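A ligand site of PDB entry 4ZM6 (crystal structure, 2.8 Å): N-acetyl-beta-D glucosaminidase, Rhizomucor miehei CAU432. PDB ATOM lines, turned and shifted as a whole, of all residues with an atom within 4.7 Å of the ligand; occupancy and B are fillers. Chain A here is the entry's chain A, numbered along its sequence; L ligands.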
ATOM      1  N   ARG A 520     -12.846 -34.622   1.694  1.00  0.00           N
ATOM      2  CA  ARG A 520     -11.662 -33.946   1.150  1.00  0.00           C
ATOM      3  C   ARG A 520     -11.223 -34.559  -0.193  1.00  0.00           C
ATOM      4  O   ARG A 520     -10.713 -33.853  -1.070  1.00  0.00           O
ATOM      5  CB  ARG A 520     -10.529 -34.036   2.167  1.00  0.00           C
ATOM      6  CG  ARG A 520     -10.822 -33.288   3.458  1.00  0.00           C
ATOM      7  CD  ARG A 520     -10.513 -34.121   4.703  1.00  0.00           C
ATOM      8  NE  ARG A 520      -9.338 -33.688   5.470  1.00  0.00           N
ATOM      9  CZ  ARG A 520      -8.074 -33.745   5.051  1.00  0.00           C
ATOM     10  NH1 ARG A 520      -7.754 -34.183   3.837  1.00  0.00           N
ATOM     11  NH2 ARG A 520      -7.103 -33.356   5.860  1.00  0.00           N
ATOM     12  N   ILE A 560       4.761 -14.744   5.909  1.00  0.00           N
ATOM     13  CA  ILE A 560       4.959 -15.954   6.722  1.00  0.00           C
ATOM     14  C   ILE A 560       6.182 -15.881   7.637  1.00  0.00           C
ATOM     15  O   ILE A 560       6.111 -16.269   8.791  1.00  0.00           O
ATOM     16  CB  ILE A 560       5.096 -17.200   5.822  1.00  0.00           C
ATOM     17  CG1 ILE A 560       3.762 -17.485   5.139  1.00  0.00           C
ATOM     18  CG2 ILE A 560       5.579 -18.412   6.612  1.00  0.00           C
ATOM     19  CD1 ILE A 560       3.825 -18.527   4.054  1.00  0.00           C
ATOM     20  N   PHE A 561       7.308 -15.410   7.096  1.00  0.00           N
ATOM     21  CA  PHE A 561       8.590 -15.374   7.806  1.00  0.00           C
ATOM     22  C   PHE A 561       9.074 -13.955   8.148  1.00  0.00           C
ATOM     23  O   PHE A 561      10.119 -13.791   8.763  1.00  0.00           O
ATOM     24  CB  PHE A 561       9.675 -16.044   6.964  1.00  0.00           C
ATOM     25  CG  PHE A 561       9.439 -17.498   6.696  1.00  0.00           C
ATOM     26  CD1 PHE A 561       9.559 -18.430   7.713  1.00  0.00           C
ATOM     27  CD2 PHE A 561       9.160 -17.956   5.404  1.00  0.00           C
ATOM     28  CE1 PHE A 561       9.366 -19.786   7.474  1.00  0.00           C
ATOM     29  CE2 PHE A 561       8.971 -19.299   5.155  1.00  0.00           C
ATOM     30  CZ  PHE A 561       9.066 -20.216   6.188  1.00  0.00           C
ATOM     31  N   LEU A 613      14.657 -30.335  -0.553  1.00  0.00           N
ATOM     32  CA  LEU A 613      13.432 -29.556  -0.471  1.00  0.00           C
ATOM     33  C   LEU A 613      13.811 -28.244   0.211  1.00  0.00           C
ATOM     34  O   LEU A 613      13.854 -28.159   1.431  1.00  0.00           O
ATOM     35  CB  LEU A 613      12.344 -30.310   0.292  1.00  0.00           C
ATOM     36  CG  LEU A 613      10.893 -29.886   0.055  1.00  0.00           C
ATOM     37  CD1 LEU A 613       9.919 -30.854   0.714  1.00  0.00           C
ATOM     38  CD2 LEU A 613      10.627 -28.496   0.587  1.00  0.00           C
ATOM     39  N   MET A 614      14.104 -27.237  -0.608  1.00  0.00           N
ATOM     40  CA  MET A 614      14.689 -25.992  -0.128  1.00  0.00           C
ATOM     41  C   MET A 614      13.690 -25.207   0.717  1.00  0.00           C
ATOM     42  O   MET A 614      14.061 -24.614   1.727  1.00  0.00           O
ATOM     43  CB  MET A 614      15.158 -25.121  -1.303  1.00  0.00           C
ATOM     44  CG  MET A 614      16.228 -25.751  -2.179  1.00  0.00           C
ATOM     45  SD  MET A 614      16.504 -24.811  -3.701  1.00  0.00           S
ATOM     46  CE  MET A 614      17.292 -23.343  -3.043  1.00  0.00           C
ATOM     47  N   LEU A 615      12.451 -25.190   0.283  1.00  0.00           N
ATOM     48  CA  LEU A 615      11.429 -24.417   0.964  1.00  0.00           C
ATOM     49  C   LEU A 615      10.038 -24.927   0.592  1.00  0.00           C
ATOM     50  O   LEU A 615       9.822 -25.387  -0.535  1.00  0.00           O
ATOM     51  CB  LEU A 615      11.557 -22.941   0.590  1.00  0.00           C
ATOM     52  CG  LEU A 615      10.666 -21.946   1.335  1.00  0.00           C
ATOM     53  CD1 LEU A 615      11.166 -21.746   2.755  1.00  0.00           C
ATOM     54  CD2 LEU A 615      10.638 -20.613   0.605  1.00  0.00           C
ATOM     55  N   LEU A 616       9.134 -24.880   1.563  1.00  0.00           N
ATOM     56  CA  LEU A 616       7.728 -25.172   1.346  1.00  0.00           C
ATOM     57  C   LEU A 616       6.965 -24.186   2.210  1.00  0.00           C
ATOM     58  O   LEU A 616       7.226 -24.101   3.406  1.00  0.00           O
ATOM     59  CB  LEU A 616       7.402 -26.606   1.797  1.00  0.00           C
ATOM     60  CG  LEU A 616       6.249 -27.373   1.130  1.00  0.00           C
ATOM     61  CD1 LEU A 616       5.615 -28.333   2.151  1.00  0.00           C
ATOM     62  CD2 LEU A 616       5.178 -26.472   0.531  1.00  0.00           C
ATOM     63  N   MET A 617       6.060 -23.431   1.610  1.00  0.00           N
ATOM     64  CA  MET A 617       5.314 -22.408   2.353  1.00  0.00           C
ATOM     65  C   MET A 617       3.977 -22.133   1.673  1.00  0.00           C
ATOM     66  O   MET A 617       3.892 -22.147   0.448  1.00  0.00           O
ATOM     67  CB  MET A 617       6.129 -21.109   2.425  1.00  0.00           C
ATOM     68  CG  MET A 617       6.117 -20.288   1.142  1.00  0.00           C
ATOM     69  SD  MET A 617       7.339 -18.956   1.008  1.00  0.00           S
ATOM     70  CE  MET A 617       7.119 -18.133   2.580  1.00  0.00           C
ATOM     71  N   VAL A 618       2.938 -21.903   2.481  1.00  0.00           N
ATOM     72  CA  VAL A 618       1.638 -21.474   1.959  1.00  0.00           C
ATOM     73  C   VAL A 618       1.057 -20.358   2.842  1.00  0.00           C
ATOM     74  O   VAL A 618       1.275 -20.330   4.052  1.00  0.00           O
ATOM     75  CB  VAL A 618       0.621 -22.651   1.771  1.00  0.00           C
ATOM     76  CG1 VAL A 618       1.307 -24.006   1.857  1.00  0.00           C
ATOM     77  CG2 VAL A 618      -0.510 -22.608   2.786  1.00  0.00           C
ATOM     78  N   TYR A 622      -4.712 -19.613   3.801  1.00  0.00           N
ATOM     79  CA  TYR A 622      -4.948 -20.805   2.987  1.00  0.00           C
ATOM     80  C   TYR A 622      -4.368 -22.117   3.558  1.00  0.00           C
ATOM     81  O   TYR A 622      -4.516 -23.177   2.947  1.00  0.00           O
ATOM     82  CB  TYR A 622      -4.394 -20.553   1.586  1.00  0.00           C
ATOM     83  CG  TYR A 622      -5.258 -19.634   0.766  1.00  0.00           C
ATOM     84  CD1 TYR A 622      -5.135 -18.252   0.877  1.00  0.00           C
ATOM     85  CD2 TYR A 622      -6.202 -20.141  -0.113  1.00  0.00           C
ATOM     86  CE1 TYR A 622      -5.921 -17.404   0.120  1.00  0.00           C
ATOM     87  CE2 TYR A 622      -7.001 -19.311  -0.871  1.00  0.00           C
ATOM     88  CZ  TYR A 622      -6.860 -17.938  -0.752  1.00  0.00           C
ATOM     89  OH  TYR A 622      -7.660 -17.131  -1.509  1.00  0.00           O
ATOM     90  N   GLN A 623      -3.727 -22.041   4.719  1.00  0.00           N
ATOM     91  CA  GLN A 623      -3.235 -23.255   5.383  1.00  0.00           C
ATOM     92  C   GLN A 623      -4.387 -24.143   5.865  1.00  0.00           C
ATOM     93  O   GLN A 623      -5.504 -23.664   6.054  1.00  0.00           O
ATOM     94  CB  GLN A 623      -2.292 -22.882   6.542  1.00  0.00           C
ATOM     95  CG  GLN A 623      -0.977 -22.320   6.031  1.00  0.00           C
ATOM     96  CD  GLN A 623      -0.084 -21.732   7.109  1.00  0.00           C
ATOM     97  OE1 GLN A 623      -0.247 -21.996   8.289  1.00  0.00           O
ATOM     98  NE2 GLN A 623       0.886 -20.933   6.679  1.00  0.00           N
ATOM     99  N   GLY A 624      -4.112 -25.426   6.024  1.00  0.00           N
ATOM    100  CA  GLY A 624      -5.120 -26.394   6.463  1.00  0.00           C
ATOM    101  C   GLY A 624      -6.176 -26.740   5.432  1.00  0.00           C
ATOM    102  O   GLY A 624      -7.283 -27.171   5.779  1.00  0.00           O
ATOM    103  N   LYS A 625      -5.850 -26.553   4.152  1.00  0.00           N
ATOM    104  CA  LYS A 625      -6.767 -26.913   3.054  1.00  0.00           C
ATOM    105  C   LYS A 625      -6.160 -27.960   2.105  1.00  0.00           C
ATOM    106  O   LYS A 625      -6.778 -28.297   1.090  1.00  0.00           O
ATOM    107  CB  LYS A 625      -7.155 -25.667   2.264  1.00  0.00           C
ATOM    108  CG  LYS A 625      -7.761 -24.560   3.104  1.00  0.00           C
ATOM    109  CD  LYS A 625      -8.125 -23.356   2.252  1.00  0.00           C
ATOM    110  CE  LYS A 625      -8.723 -22.227   3.085  1.00  0.00           C
ATOM    111  NZ  LYS A 625     -10.019 -22.626   3.686  1.00  0.00           N
ATOM    112  N   GLY A 626      -4.970 -28.457   2.428  1.00  0.00           N
ATOM    113  CA  GLY A 626      -4.300 -29.467   1.597  1.00  0.00           C
ATOM    114  C   GLY A 626      -3.371 -28.904   0.521  1.00  0.00           C
ATOM    115  O   GLY A 626      -2.880 -29.660  -0.314  1.00  0.00           O
ATOM    116  N   VAL A 627      -3.114 -27.593   0.545  1.00  0.00           N
ATOM    117  CA  VAL A 627      -2.220 -26.974  -0.435  1.00  0.00           C
ATOM    118  C   VAL A 627      -0.773 -27.389  -0.188  1.00  0.00           C
ATOM    119  O   VAL A 627      -0.050 -27.731  -1.125  1.00  0.00           O
ATOM    120  CB  VAL A 627      -2.318 -25.437  -0.417  1.00  0.00           C
ATOM    121  CG1 VAL A 627      -1.288 -24.814  -1.349  1.00  0.00           C
ATOM    122  CG2 VAL A 627      -3.720 -24.989  -0.798  1.00  0.00           C
ATOM    123  N   GLY A 628      -0.353 -27.337   1.071  1.00  0.00           N
ATOM    124  CA  GLY A 628       0.982 -27.783   1.451  1.00  0.00           C
ATOM    125  C   GLY A 628       1.249 -29.190   0.935  1.00  0.00           C
ATOM    126  O   GLY A 628       2.327 -29.483   0.419  1.00  0.00           O
ATOM    127  N   THR A 629       0.238 -30.039   1.075  1.00  0.00           N
ATOM    128  CA  THR A 629       0.339 -31.440   0.674  1.00  0.00           C
ATOM    129  C   THR A 629       0.430 -31.588  -0.846  1.00  0.00           C
ATOM    130  O   THR A 629       1.217 -32.401  -1.339  1.00  0.00           O
ATOM    131  CB  THR A 629      -0.850 -32.236   1.247  1.00  0.00           C
ATOM    132  OG1 THR A 629      -0.698 -32.319   2.675  1.00  0.00           O
ATOM    133  CG2 THR A 629      -0.892 -33.651   0.681  1.00  0.00           C
ATOM    134  N   LEU A 649      15.442 -32.208   4.042  1.00  0.00           N
ATOM    135  CA  LEU A 649      14.669 -31.009   4.382  1.00  0.00           C
ATOM    136  C   LEU A 649      15.629 -29.828   4.488  1.00  0.00           C
ATOM    137  O   LEU A 649      16.600 -29.883   5.256  1.00  0.00           O
ATOM    138  CB  LEU A 649      13.905 -31.159   5.705  1.00  0.00           C
ATOM    139  CG  LEU A 649      12.581 -31.923   5.726  1.00  0.00           C
ATOM    140  CD1 LEU A 649      11.956 -31.807   7.105  1.00  0.00           C
ATOM    141  CD2 LEU A 649      11.615 -31.408   4.669  1.00  0.00           C
ATOM    142  N   GLY A 650      15.336 -28.776   3.740  1.00  0.00           N
ATOM    143  CA  GLY A 650      16.247 -27.639   3.610  1.00  0.00           C
ATOM    144  C   GLY A 650      17.270 -27.950   2.542  1.00  0.00           C
ATOM    145  O   GLY A 650      17.141 -28.941   1.813  1.00  0.00           O
ATOM    146  N   PHE A 657      17.184 -22.308   4.544  1.00  0.00           N
ATOM    147  CA  PHE A 657      17.387 -23.012   5.814  1.00  0.00           C
ATOM    148  C   PHE A 657      18.084 -24.356   5.577  1.00  0.00           C
ATOM    149  O   PHE A 657      17.863 -24.993   4.543  1.00  0.00           O
ATOM    150  CB  PHE A 657      16.045 -23.261   6.508  1.00  0.00           C
ATOM    151  CG  PHE A 657      15.173 -22.036   6.656  1.00  0.00           C
ATOM    152  CD1 PHE A 657      15.631 -20.923   7.347  1.00  0.00           C
ATOM    153  CD2 PHE A 657      13.880 -22.005   6.144  1.00  0.00           C
ATOM    154  CE1 PHE A 657      14.829 -19.793   7.504  1.00  0.00           C
ATOM    155  CE2 PHE A 657      13.072 -20.894   6.295  1.00  0.00           C
ATOM    156  CZ  PHE A 657      13.545 -19.781   6.973  1.00  0.00           C
ATOM    157  N   GLY A 659      17.743 -26.892   7.749  1.00  0.00           N
ATOM    158  CA  GLY A 659      16.750 -27.837   8.235  1.00  0.00           C
ATOM    159  C   GLY A 659      15.497 -27.040   8.513  1.00  0.00           C
ATOM    160  O   GLY A 659      15.243 -26.046   7.826  1.00  0.00           O
ATOM    161  N   VAL A 660      14.732 -27.443   9.510  1.00  0.00           N
ATOM    162  CA  VAL A 660      13.499 -26.735   9.830  1.00  0.00           C
ATOM    163  C   VAL A 660      13.717 -25.866  11.063  1.00  0.00           C
ATOM    164  O   VAL A 660      14.096 -26.363  12.115  1.00  0.00           O
ATOM    165  CB  VAL A 660      12.325 -27.699  10.077  1.00  0.00           C
ATOM    166  CG1 VAL A 660      11.036 -26.920  10.314  1.00  0.00           C
ATOM    167  CG2 VAL A 660      12.166 -28.653   8.900  1.00  0.00           C
ATOM    168  N   PRO A 661      13.493 -24.544  10.930  1.00  0.00           N
ATOM    169  CA  PRO A 661      13.605 -23.638  12.071  1.00  0.00           C
ATOM    170  C   PRO A 661      12.900 -24.194  13.313  1.00  0.00           C
ATOM    171  O   PRO A 661      11.920 -24.927  13.194  1.00  0.00           O
ATOM    172  CB  PRO A 661      12.894 -22.376  11.580  1.00  0.00           C
ATOM    173  CG  PRO A 661      13.076 -22.390  10.099  1.00  0.00           C
ATOM    174  CD  PRO A 661      13.173 -23.828   9.678  1.00  0.00           C
ATOM    175  N   GLN A 666       4.992 -21.740  14.709  1.00  0.00           N
ATOM    176  CA  GLN A 666       4.612 -22.103  13.344  1.00  0.00           C
ATOM    177  C   GLN A 666       5.668 -22.993  12.676  1.00  0.00           C
ATOM    178  O   GLN A 666       5.327 -23.887  11.882  1.00  0.00           O
ATOM    179  CB  GLN A 666       4.346 -20.857  12.496  1.00  0.00           C
ATOM    180  N   SER A 667       6.934 -22.772  13.008  1.00  0.00           N
ATOM    181  CA  SER A 667       8.012 -23.610  12.486  1.00  0.00           C
ATOM    182  C   SER A 667       8.019 -25.008  13.104  1.00  0.00           C
ATOM    183  O   SER A 667       8.126 -25.991  12.371  1.00  0.00           O
ATOM    184  CB  SER A 667       9.365 -22.941  12.701  1.00  0.00           C
ATOM    185  OG  SER A 667       9.484 -21.792  11.873  1.00  0.00           O
ATOM    186  N   ALA A 670       5.414 -26.964  11.614  1.00  0.00           N
ATOM    187  CA  ALA A 670       5.846 -27.450  10.302  1.00  0.00           C
ATOM    188  C   ALA A 670       6.778 -28.662  10.405  1.00  0.00           C
ATOM    189  O   ALA A 670       6.867 -29.456   9.475  1.00  0.00           O
ATOM    190  CB  ALA A 670       6.518 -26.348   9.502  1.00  0.00           C
ATOM    191  N   PHE A 673       4.380 -31.474  10.668  1.00  0.00           N
ATOM    192  CA  PHE A 673       3.841 -31.695   9.342  1.00  0.00           C
ATOM    193  C   PHE A 673       4.725 -32.672   8.556  1.00  0.00           C
ATOM    194  O   PHE A 673       4.225 -33.644   7.978  1.00  0.00           O
ATOM    195  CB  PHE A 673       3.715 -30.364   8.590  1.00  0.00           C
ATOM    196  CG  PHE A 673       3.344 -30.519   7.135  1.00  0.00           C
ATOM    197  CD1 PHE A 673       4.330 -30.675   6.171  1.00  0.00           C
ATOM    198  CD2 PHE A 673       2.023 -30.499   6.743  1.00  0.00           C
ATOM    199  CE1 PHE A 673       3.990 -30.819   4.842  1.00  0.00           C
ATOM    200  CE2 PHE A 673       1.674 -30.647   5.404  1.00  0.00           C
ATOM    201  CZ  PHE A 673       2.661 -30.798   4.457  1.00  0.00           C
ATOM    202  N   PHE A 674       6.029 -32.405   8.565  1.00  0.00           N
ATOM    203  CA  PHE A 674       6.992 -33.201   7.787  1.00  0.00           C
ATOM    204  C   PHE A 674       7.206 -34.613   8.337  1.00  0.00           C
ATOM    205  O   PHE A 674       7.249 -35.568   7.560  1.00  0.00           O
ATOM    206  CB  PHE A 674       8.331 -32.467   7.647  1.00  0.00           C
ATOM    207  CG  PHE A 674       8.279 -31.276   6.712  1.00  0.00           C
ATOM    208  CD1 PHE A 674       7.895 -31.419   5.393  1.00  0.00           C
ATOM    209  CD2 PHE A 674       8.642 -30.022   7.166  1.00  0.00           C
ATOM    210  CE1 PHE A 674       7.841 -30.333   4.537  1.00  0.00           C
ATOM    211  CE2 PHE A 674       8.605 -28.933   6.314  1.00  0.00           C
ATOM    212  CZ  PHE A 674       8.196 -29.079   4.997  1.00  0.00           C
ATOM    213  N   LYS A 676       5.115 -36.373  10.111  1.00  0.00           N
ATOM    214  CA  LYS A 676       3.853 -37.062   9.865  1.00  0.00           C
ATOM    215  C   LYS A 676       3.709 -37.610   8.443  1.00  0.00           C
ATOM    216  O   LYS A 676       2.976 -38.583   8.222  1.00  0.00           O
ATOM    217  CB  LYS A 676       2.686 -36.128  10.174  1.00  0.00           C
ATOM    218  CG  LYS A 676       1.362 -36.838  10.390  1.00  0.00           C
ATOM    219  CD  LYS A 676       0.591 -36.156  11.517  1.00  0.00           C
ATOM    220  CE  LYS A 676      -0.678 -36.915  11.845  1.00  0.00           C
ATOM    221  NZ  LYS A 676      -1.604 -36.989  10.677  1.00  0.00           N
HETATM  222  N1  LIG L   1     -10.143 -30.385   6.244  1.00  0.00           N
HETATM  223  C1  LIG L   1      -9.700 -30.607   7.495  1.00  0.00           C
HETATM  224  N2  LIG L   1      -8.391 -30.687   7.814  1.00  0.00           N
HETATM  225  C2  LIG L   1      -7.426 -30.520   6.874  1.00  0.00           C
HETATM  226  C3  LIG L   1      -7.845 -30.279   5.483  1.00  0.00           C
HETATM  227  C4  LIG L   1      -9.296 -30.218   5.199  1.00  0.00           C
HETATM  228  N3  LIG L   1      -9.738 -29.991   3.935  1.00  0.00           N
HETATM  229  N4  LIG L   1      -6.723 -30.164   4.755  1.00  0.00           N
HETATM  230  C5  LIG L   1      -5.670 -30.322   5.606  1.00  0.00           C
HETATM  231  N5  LIG L   1      -6.089 -30.539   6.872  1.00  0.00           N
HETATM  232  C6  LIG L   1      -5.195 -30.746   8.045  1.00  0.00           C
HETATM  233  C7  LIG L   1      -4.942 -32.231   8.324  1.00  0.00           C
HETATM  234  O1  LIG L   1      -5.103 -32.496   9.721  1.00  0.00           O
HETATM  235  C8  LIG L   1      -3.522 -32.508   7.835  1.00  0.00           C
HETATM  236  O2  LIG L   1      -2.801 -33.451   8.644  1.00  0.00           O
HETATM  237  P1  LIG L   1      -2.151 -33.208  10.112  1.00  0.00           P
HETATM  238  O3  LIG L   1      -0.790 -32.607   9.851  1.00  0.00           O
HETATM  239  O4  LIG L   1      -3.134 -32.323  10.848  1.00  0.00           O
HETATM  240  O5  LIG L   1      -2.090 -34.603  10.670  1.00  0.00           O
HETATM  241  C9  LIG L   1      -2.880 -31.136   7.750  1.00  0.00           C
HETATM  242  O6  LIG L   1      -3.925 -30.147   7.787  1.00  0.00           O
HETATM  243  C10 LIG L   1      -2.037 -30.990   6.488  1.00  0.00           C
HETATM  244  O7  LIG L   1      -1.997 -29.616   6.138  1.00  0.00           O
HETATM  245  P2  LIG L   1      -2.025 -29.108   4.621  1.00  0.00           P
HETATM  246  O8  LIG L   1      -3.246 -28.244   4.461  1.00  0.00           O
HETATM  247  O9  LIG L   1      -1.770 -30.237   3.653  1.00  0.00           O
HETATM  248  O10 LIG L   1      -0.682 -28.239   4.725  1.00  0.00           O
HETATM  249  P3  LIG L   1      -0.733 -26.636   4.733  1.00  0.00           P
HETATM  250  O11 LIG L   1      -1.407 -26.200   3.451  1.00  0.00           O
HETATM  251  O12 LIG L   1      -1.285 -26.152   6.043  1.00  0.00           O
HETATM  252  O13 LIG L   1       0.833 -26.313   4.674  1.00  0.00           O
HETATM  253  C11 LIG L   1       2.878 -25.898   5.894  1.00  0.00           C
HETATM  254  C12 LIG L   1       1.706 -26.840   5.670  1.00  0.00           C
HETATM  255  C13 LIG L   1       3.696 -25.761   4.618  1.00  0.00           C
HETATM  256  C14 LIG L   1       3.769 -26.496   6.974  1.00  0.00           C
HETATM  257  C15 LIG L   1       2.297 -24.553   6.326  1.00  0.00           C
HETATM  258  O14 LIG L   1       1.876 -24.625   7.689  1.00  0.00           O
HETATM  259  C16 LIG L   1       3.244 -23.404   6.159  1.00  0.00           C
HETATM  260  O15 LIG L   1       3.184 -22.725   5.132  1.00  0.00           O
HETATM  261  N6  LIG L   1       4.114 -23.140   7.133  1.00  0.00           N
HETATM  262  C17 LIG L   1       5.012 -21.997   7.032  1.00  0.00           C
HETATM  263  C18 LIG L   1       6.133 -22.037   8.048  1.00  0.00           C
HETATM  264  C19 LIG L   1       7.178 -23.119   7.834  1.00  0.00           C
HETATM  265  O16 LIG L   1       7.768 -23.493   8.832  1.00  0.00           O
HETATM  266  N7  LIG L   1       7.464 -23.610   6.613  1.00  0.00           N
HETATM  267  C20 LIG L   1       8.533 -24.603   6.407  1.00  0.00           C
HETATM  268  C21 LIG L   1       9.885 -23.967   6.089  1.00  0.00           C
HETATM  269  S1  LIG L   1      11.251 -25.068   6.366  1.00  0.00           S
HETATM  270  C22 LIG L   1      11.467 -25.853   4.911  1.00  0.00           C
HETATM  271  O17 LIG L   1      10.688 -25.666   3.993  1.00  0.00           O
HETATM  272  C23 LIG L   1      12.622 -26.788   4.801  1.00  0.00           C
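Ile 560 touches the ligand (CG2 to C17, 3.7 Å).
Phe 561 touches the ligand.
Leu 613 touches the ligand (O to C23, 3.8 Å).
CA of Leu 615 touches O17 of the ligand, 3.4 Å away.
Met 617 touches the ligand (CA to O15, 3.5 Å).
Val 627 touches the ligand.
N of Gly 650 touches C23 of the ligand (3.5 Å).
O of Gln 666 touches O16 of the ligand, 3.9 Å away.
Ser 667 touches the ligand (CA to O16, 3.7 Å).
CB of Ala 670 touches O16 of the ligand, at 3.2 Å.
CE2 of Phe 673 touches O10 of the ligand (3.4 Å).
O of Leu 613 lies within hydrogen-bond range of N of Gly 650, 2.8 Å away.
The backbone carbonyl oxygen (O) of Val 618 lies within hydrogen-bond range of the side-chain amide nitrogen (NE2) of Gln 623, at 2.7 Å.
The side-chain amide nitrogen (NE2) of Gln 623 lies within hydrogen-bond range of an oxygen (O15) of the ligand (3.3 Å).
N of Gly 628 sits at hydrogen-bond distance from O11 of the ligand, 2.8 Å away.
An oxygen (O9) of the ligand lies close to the backbone NH (N) of Thr 629.
N of Gly 626 sits at hydrogen-bond distance from O8 of the ligand (2.7 Å).
O12 of the ligand lies within hydrogen-bond range of N of Gly 624, at 2.9 Å.
The backbone NH (N) of Leu 616 lies within hydrogen-bond range of an oxygen (O17) of the ligand, at 3.0 Å.
A nitrogen (N4) of the ligand sits close to the guanidinium group (NH2) of Arg 520, 3.4 Å away.
NZ of Lys 676 lies within salt-bridge range of O5 of the ligand (2.4 Å).
N7 of the ligand sits at hydrogen-bond distance from O of Leu 616.
An oxygen (O9) of the ligand sits at hydrogen-bond distance from the side-chain hydroxyl (OG1) of Thr 629, at 2.5 Å.
The backbone NH of Lys 625 sits at hydrogen-bond distance from an oxygen (O8) of the ligand (3.1 Å).
An oxygen (O15) of the ligand sits at hydrogen-bond distance from the backbone NH (N) of Val 618.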
